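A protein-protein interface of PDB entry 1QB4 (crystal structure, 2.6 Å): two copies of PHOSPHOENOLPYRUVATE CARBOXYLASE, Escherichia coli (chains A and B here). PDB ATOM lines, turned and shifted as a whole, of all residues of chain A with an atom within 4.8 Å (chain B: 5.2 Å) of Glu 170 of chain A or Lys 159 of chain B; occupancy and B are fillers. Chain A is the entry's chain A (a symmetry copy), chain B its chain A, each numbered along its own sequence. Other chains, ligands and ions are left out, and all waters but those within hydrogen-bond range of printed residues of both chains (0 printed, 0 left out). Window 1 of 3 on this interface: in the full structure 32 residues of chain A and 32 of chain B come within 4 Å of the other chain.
The side-chain carboxylate (OE1) of Glu 170 of chain A is in salt-bridge range of the side-chain amino group (NZ) of Lys 159 of chain B, 3.9 Å away.
The backbone NH of Ala 167 of chain A is in hydrogen-bond range of the side-chain carboxylate of Glu 170 of chain A (2.9 Å).
CB of Pro 93 of chain B touches CB of Ala 167 of chain A, at 3.3 Å.
CB of Pro 93 of chain B touches OH of Tyr 169 of chain A, 3.0 Å away.
Pro 93 of chain B touches Glu 170 of chain A (CG to OE2, 3.3 Å).
Printed residues of chain B within 4 Å of Ala 167 of chain A: Pro 93.
Asp 168 of chain A touches none of the printed residues of chain B.
Printed residues of chain B within 4 Å of Tyr 169 of chain A: Pro 93.
Of the printed residues of chain B, Glu 170 of chain A touches Pro 93 (3.3 Å) and Lys 159 (3.8 Å).
Of the printed residues of chain A, Pro 93 of chain B touches Ala 167, Tyr 169 and Glu 170.
Lys 159 of chain B touches just one residue of chain A: Glu 170 (3.8 Å).
Asp 162 of chain B touches none of the printed residues of chain A.
The nearest printed residue of chain B that does not touch Ala 167 of chain A is Lys 159 of chain B (8.7 Å).
Hydrophobic or aromatic side chains of chain A within 4 Å of the printed part of chain B: Ala 167 and Tyr 169.
Along chain A the printed residues that touch a printed residue of chain B span positions 167 to 170.
Among the printed residues, 4 pairs touch across the chains.
No position is printed for both chains.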
ATOM      1  N   ASP A 165     -15.840   1.881   7.771  1.00  0.00           N
ATOM      2  CA  ASP A 165     -14.857   1.484   8.797  1.00  0.00           C
ATOM      3  C   ASP A 165     -15.504   1.404  10.173  1.00  0.00           C
ATOM      4  O   ASP A 165     -14.788   1.610  11.177  1.00  0.00           O
ATOM      5  CB  ASP A 165     -13.671   2.450   8.840  1.00  0.00           C
ATOM      6  CG  ASP A 165     -12.867   2.750   7.608  1.00  0.00           C
ATOM      7  OD1 ASP A 165     -12.618   1.867   6.746  1.00  0.00           O
ATOM      8  OD2 ASP A 165     -12.442   3.938   7.448  1.00  0.00           O
ATOM      9  N   ILE A 166     -16.817   1.158  10.356  1.00  0.00           N
ATOM     10  CA  ILE A 166     -17.255   1.083  11.741  1.00  0.00           C
ATOM     11  C   ILE A 166     -17.073  -0.413  12.127  1.00  0.00           C
ATOM     12  O   ILE A 166     -17.526  -1.261  11.380  1.00  0.00           O
ATOM     13  CB  ILE A 166     -18.537   1.608  12.298  1.00  0.00           C
ATOM     14  CG1 ILE A 166     -19.820   1.172  11.623  1.00  0.00           C
ATOM     15  CG2 ILE A 166     -18.466   3.144  12.421  1.00  0.00           C
ATOM     16  CD1 ILE A 166     -20.994   1.400  12.570  1.00  0.00           C
ATOM     17  N   ALA A 167     -16.360  -0.557  13.228  1.00  0.00           N
ATOM     18  CA  ALA A 167     -16.074  -1.884  13.766  1.00  0.00           C
ATOM     19  C   ALA A 167     -17.382  -2.644  13.882  1.00  0.00           C
ATOM     20  O   ALA A 167     -18.407  -2.150  14.410  1.00  0.00           O
ATOM     21  CB  ALA A 167     -15.395  -1.746  15.135  1.00  0.00           C
ATOM     22  N   ASP A 168     -17.396  -3.892  13.440  1.00  0.00           N
ATOM     23  CA  ASP A 168     -18.632  -4.649  13.513  1.00  0.00           C
ATOM     24  C   ASP A 168     -19.355  -4.613  14.838  1.00  0.00           C
ATOM     25  O   ASP A 168     -20.594  -4.660  14.799  1.00  0.00           O
ATOM     26  CB  ASP A 168     -18.473  -6.088  13.042  1.00  0.00           C
ATOM     27  CG  ASP A 168     -17.129  -6.703  13.296  1.00  0.00           C
ATOM     28  OD1 ASP A 168     -16.905  -7.406  14.296  1.00  0.00           O
ATOM     29  OD2 ASP A 168     -16.224  -6.453  12.442  1.00  0.00           O
ATOM     30  N   TYR A 169     -18.704  -4.547  15.979  1.00  0.00           N
ATOM     31  CA  TYR A 169     -19.359  -4.524  17.276  1.00  0.00           C
ATOM     32  C   TYR A 169     -20.088  -3.213  17.457  1.00  0.00           C
ATOM     33  O   TYR A 169     -21.161  -3.263  18.032  1.00  0.00           O
ATOM     34  CB  TYR A 169     -18.461  -4.800  18.463  1.00  0.00           C
ATOM     35  CG  TYR A 169     -17.177  -4.033  18.584  1.00  0.00           C
ATOM     36  CD1 TYR A 169     -17.015  -3.055  19.561  1.00  0.00           C
ATOM     37  CD2 TYR A 169     -16.106  -4.295  17.727  1.00  0.00           C
ATOM     38  CE1 TYR A 169     -15.824  -2.359  19.666  1.00  0.00           C
ATOM     39  CE2 TYR A 169     -14.910  -3.607  17.835  1.00  0.00           C
ATOM     40  CZ  TYR A 169     -14.790  -2.633  18.802  1.00  0.00           C
ATOM     41  OH  TYR A 169     -13.627  -1.925  18.914  1.00  0.00           O
ATOM     42  N   GLU A 170     -19.473  -2.129  16.961  1.00  0.00           N
ATOM     43  CA  GLU A 170     -20.156  -0.821  17.096  1.00  0.00           C
ATOM     44  C   GLU A 170     -21.456  -0.886  16.280  1.00  0.00           C
ATOM     45  O   GLU A 170     -22.527  -0.551  16.766  1.00  0.00           O
ATOM     46  CB  GLU A 170     -19.353   0.346  16.572  1.00  0.00           C
ATOM     47  CG  GLU A 170     -18.032   0.564  17.330  1.00  0.00           C
ATOM     48  CD  GLU A 170     -17.256   1.594  16.506  1.00  0.00           C
ATOM     49  OE1 GLU A 170     -17.436   2.787  16.809  1.00  0.00           O
ATOM     50  OE2 GLU A 170     -16.533   1.161  15.586  1.00  0.00           O
ATOM     51  N   HIS A 171     -21.302  -1.417  15.080  1.00  0.00           N
ATOM     52  CA  HIS A 171     -22.405  -1.587  14.168  1.00  0.00           C
ATOM     53  C   HIS A 171     -23.553  -2.354  14.763  1.00  0.00           C
ATOM     54  O   HIS A 171     -24.735  -2.101  14.662  1.00  0.00           O
ATOM     55  CB  HIS A 171     -21.949  -2.351  12.930  1.00  0.00           C
ATOM     56  CG  HIS A 171     -23.000  -2.293  11.865  1.00  0.00           C
ATOM     57  ND1 HIS A 171     -24.014  -3.225  11.771  1.00  0.00           N
ATOM     58  CD2 HIS A 171     -23.188  -1.395  10.860  1.00  0.00           C
ATOM     59  CE1 HIS A 171     -24.790  -2.914  10.738  1.00  0.00           C
ATOM     60  NE2 HIS A 171     -24.319  -1.804  10.184  1.00  0.00           N
ATOM     61  N   ASN A 172     -23.184  -3.411  15.438  1.00  0.00           N
ATOM     62  CA  ASN A 172     -24.126  -4.296  16.107  1.00  0.00           C
ATOM     63  C   ASN A 172     -24.855  -3.548  17.213  1.00  0.00           C
ATOM     64  O   ASN A 172     -26.073  -3.700  17.392  1.00  0.00           O
ATOM     65  CB  ASN A 172     -23.213  -5.424  16.640  1.00  0.00           C
ATOM     66  CG  ASN A 172     -24.047  -6.573  17.164  1.00  0.00           C
ATOM     67  OD1 ASN A 172     -24.550  -6.524  18.302  1.00  0.00           O
ATOM     68  ND2 ASN A 172     -24.174  -7.542  16.261  1.00  0.00           N
ATOM     69  N   GLN A 173     -24.122  -2.740  17.977  1.00  0.00           N
ATOM     70  CA  GLN A 173     -24.657  -1.965  19.095  1.00  0.00           C
ATOM     71  C   GLN A 173     -25.702  -0.942  18.624  1.00  0.00           C
ATOM     72  O   GLN A 173     -26.812  -0.840  19.160  1.00  0.00           O
ATOM     73  CB  GLN A 173     -23.540  -1.309  19.884  1.00  0.00           C
ATOM     74  CG  GLN A 173     -22.712  -2.203  20.742  1.00  0.00           C
ATOM     75  CD  GLN A 173     -21.364  -1.741  21.214  1.00  0.00           C
ATOM     76  OE1 GLN A 173     -20.969  -0.585  21.239  1.00  0.00           O
ATOM     77  NE2 GLN A 173     -20.483  -2.654  21.658  1.00  0.00           N
ATOM     78  N   LEU A 174     -25.292  -0.232  17.562  1.00  0.00           N
ATOM     79  CA  LEU A 174     -26.132   0.770  16.898  1.00  0.00           C
ATOM     80  C   LEU A 174     -27.400   0.122  16.377  1.00  0.00           C
ATOM     81  O   LEU A 174     -28.531   0.496  16.667  1.00  0.00           O
ATOM     82  CB  LEU A 174     -25.330   1.385  15.758  1.00  0.00           C
ATOM     83  CG  LEU A 174     -24.283   2.417  16.196  1.00  0.00           C
ATOM     84  CD1 LEU A 174     -23.642   3.024  14.988  1.00  0.00           C
ATOM     85  CD2 LEU A 174     -24.911   3.446  17.116  1.00  0.00           C
ATOM     86  N   TYR B  88      -7.763   7.039  24.529  1.00  0.00           N
ATOM     87  CA  TYR B  88      -8.678   6.937  23.414  1.00  0.00           C
ATOM     88  C   TYR B  88      -8.292   5.768  22.506  1.00  0.00           C
ATOM     89  O   TYR B  88      -9.038   4.888  22.124  1.00  0.00           O
ATOM     90  CB  TYR B  88      -8.682   8.293  22.607  1.00  0.00           C
ATOM     91  CG  TYR B  88      -9.432   8.020  21.294  1.00  0.00           C
ATOM     92  CD1 TYR B  88     -10.791   7.730  21.382  1.00  0.00           C
ATOM     93  CD2 TYR B  88      -8.787   7.984  20.067  1.00  0.00           C
ATOM     94  CE1 TYR B  88     -11.486   7.407  20.247  1.00  0.00           C
ATOM     95  CE2 TYR B  88      -9.517   7.673  18.919  1.00  0.00           C
ATOM     96  CZ  TYR B  88     -10.836   7.384  19.008  1.00  0.00           C
ATOM     97  OH  TYR B  88     -11.632   7.086  17.930  1.00  0.00           O
ATOM     98  N   PRO B  93     -11.516   0.843  17.943  1.00  0.00           N
ATOM     99  CA  PRO B  93     -11.356  -0.376  17.165  1.00  0.00           C
ATOM    100  C   PRO B  93     -10.162  -0.356  16.232  1.00  0.00           C
ATOM    101  O   PRO B  93      -9.701  -1.443  15.846  1.00  0.00           O
ATOM    102  CB  PRO B  93     -12.669  -0.565  16.455  1.00  0.00           C
ATOM    103  CG  PRO B  93     -13.606   0.482  16.975  1.00  0.00           C
ATOM    104  CD  PRO B  93     -12.860   1.455  17.801  1.00  0.00           C
ATOM    105  N   ASN B 155     -12.933  12.774  24.809  1.00  0.00           N
ATOM    106  CA  ASN B 155     -12.910  11.480  24.227  1.00  0.00           C
ATOM    107  C   ASN B 155     -13.994  11.367  23.155  1.00  0.00           C
ATOM    108  O   ASN B 155     -13.803  10.736  22.113  1.00  0.00           O
ATOM    109  CB  ASN B 155     -13.230  10.385  25.289  1.00  0.00           C
ATOM    110  CG  ASN B 155     -13.248   8.999  24.683  1.00  0.00           C
ATOM    111  OD1 ASN B 155     -12.185   8.413  24.417  1.00  0.00           O
ATOM    112  ND2 ASN B 155     -14.357   8.394  24.362  1.00  0.00           N
ATOM    113  N   ALA B 156     -15.150  11.972  23.429  1.00  0.00           N
ATOM    114  CA  ALA B 156     -16.224  11.885  22.416  1.00  0.00           C
ATOM    115  C   ALA B 156     -15.766  12.660  21.176  1.00  0.00           C
ATOM    116  O   ALA B 156     -15.868  12.173  20.047  1.00  0.00           O
ATOM    117  CB  ALA B 156     -17.542  12.404  22.947  1.00  0.00           C
ATOM    118  N   CYS B 157     -15.183  13.838  21.420  1.00  0.00           N
ATOM    119  CA  CYS B 157     -14.677  14.636  20.320  1.00  0.00           C
ATOM    120  C   CYS B 157     -13.638  13.889  19.537  1.00  0.00           C
ATOM    121  O   CYS B 157     -13.683  13.925  18.281  1.00  0.00           O
ATOM    122  CB  CYS B 157     -14.314  16.051  20.840  1.00  0.00           C
ATOM    123  SG  CYS B 157     -15.783  17.191  20.824  1.00  0.00           S
ATOM    124  N   LEU B 158     -12.697  13.134  20.122  1.00  0.00           N
ATOM    125  CA  LEU B 158     -11.677  12.398  19.374  1.00  0.00           C
ATOM    126  C   LEU B 158     -12.299  11.260  18.569  1.00  0.00           C
ATOM    127  O   LEU B 158     -11.850  10.905  17.487  1.00  0.00           O
ATOM    128  CB  LEU B 158     -10.562  11.795  20.202  1.00  0.00           C
ATOM    129  CG  LEU B 158      -9.831  12.658  21.194  1.00  0.00           C
ATOM    130  CD1 LEU B 158      -9.134  11.815  22.254  1.00  0.00           C
ATOM    131  CD2 LEU B 158      -8.821  13.535  20.461  1.00  0.00           C
ATOM    132  N   LYS B 159     -13.320  10.676  19.165  1.00  0.00           N
ATOM    133  CA  LYS B 159     -14.040   9.594  18.507  1.00  0.00           C
ATOM    134  C   LYS B 159     -14.585  10.113  17.165  1.00  0.00           C
ATOM    135  O   LYS B 159     -14.361   9.562  16.093  1.00  0.00           O
ATOM    136  CB  LYS B 159     -15.201   9.121  19.407  1.00  0.00           C
ATOM    137  CG  LYS B 159     -16.013   8.050  18.697  1.00  0.00           C
ATOM    138  CD  LYS B 159     -16.639   7.056  19.626  1.00  0.00           C
ATOM    139  CE  LYS B 159     -17.340   5.938  18.875  1.00  0.00           C
ATOM    140  NZ  LYS B 159     -18.189   5.144  19.854  1.00  0.00           N
ATOM    141  N   GLN B 160     -15.316  11.239  17.242  1.00  0.00           N
ATOM    142  CA  GLN B 160     -15.870  11.834  16.048  1.00  0.00           C
ATOM    143  C   GLN B 160     -14.871  12.302  15.037  1.00  0.00           C
ATOM    144  O   GLN B 160     -15.124  12.159  13.826  1.00  0.00           O
ATOM    145  CB  GLN B 160     -16.824  12.958  16.441  1.00  0.00           C
ATOM    146  CG  GLN B 160     -18.082  12.281  16.989  1.00  0.00           C
ATOM    147  CD  GLN B 160     -19.044  13.299  17.549  1.00  0.00           C
ATOM    148  OE1 GLN B 160     -19.102  13.497  18.761  1.00  0.00           O
ATOM    149  NE2 GLN B 160     -19.780  13.952  16.647  1.00  0.00           N
ATOM    150  N   LEU B 161     -13.730  12.839  15.445  1.00  0.00           N
ATOM    151  CA  LEU B 161     -12.731  13.258  14.462  1.00  0.00           C
ATOM    152  C   LEU B 161     -12.099  12.065  13.785  1.00  0.00           C
ATOM    153  O   LEU B 161     -11.422  12.214  12.769  1.00  0.00           O
ATOM    154  CB  LEU B 161     -11.715  14.178  15.108  1.00  0.00           C
ATOM    155  CG  LEU B 161     -12.321  15.497  15.624  1.00  0.00           C
ATOM    156  CD1 LEU B 161     -11.520  16.061  16.780  1.00  0.00           C
ATOM    157  CD2 LEU B 161     -12.469  16.518  14.508  1.00  0.00           C
ATOM    158  N   ASP B 162     -12.303  10.852  14.285  1.00  0.00           N
ATOM    159  CA  ASP B 162     -11.738   9.652  13.708  1.00  0.00           C
ATOM    160  C   ASP B 162     -12.496   9.258  12.438  1.00  0.00           C
ATOM    161  O   ASP B 162     -11.991   8.395  11.717  1.00  0.00           O
ATOM    162  CB  ASP B 162     -11.872   8.420  14.602  1.00  0.00           C
ATOM    163  CG  ASP B 162     -10.635   7.641  14.920  1.00  0.00           C
ATOM    164  OD1 ASP B 162      -9.529   8.135  14.656  1.00  0.00           O
ATOM    165  OD2 ASP B 162     -10.728   6.514  15.474  1.00  0.00           O
ATOM    166  N   ASN B 163     -13.697   9.786  12.254  1.00  0.00           N
ATOM    167  CA  ASN B 163     -14.410   9.379  11.048  1.00  0.00           C
ATOM    168  C   ASN B 163     -13.705   9.972   9.818  1.00  0.00           C
ATOM    169  O   ASN B 163     -13.507  11.174   9.688  1.00  0.00           O
ATOM    170  CB  ASN B 163     -15.875   9.725  11.067  1.00  0.00           C
ATOM    171  CG  ASN B 163     -16.623   9.388   9.792  1.00  0.00           C
ATOM    172  OD1 ASN B 163     -17.751   9.884   9.629  1.00  0.00           O
ATOM    173  ND2 ASN B 163     -16.094   8.566   8.904  1.00  0.00           N
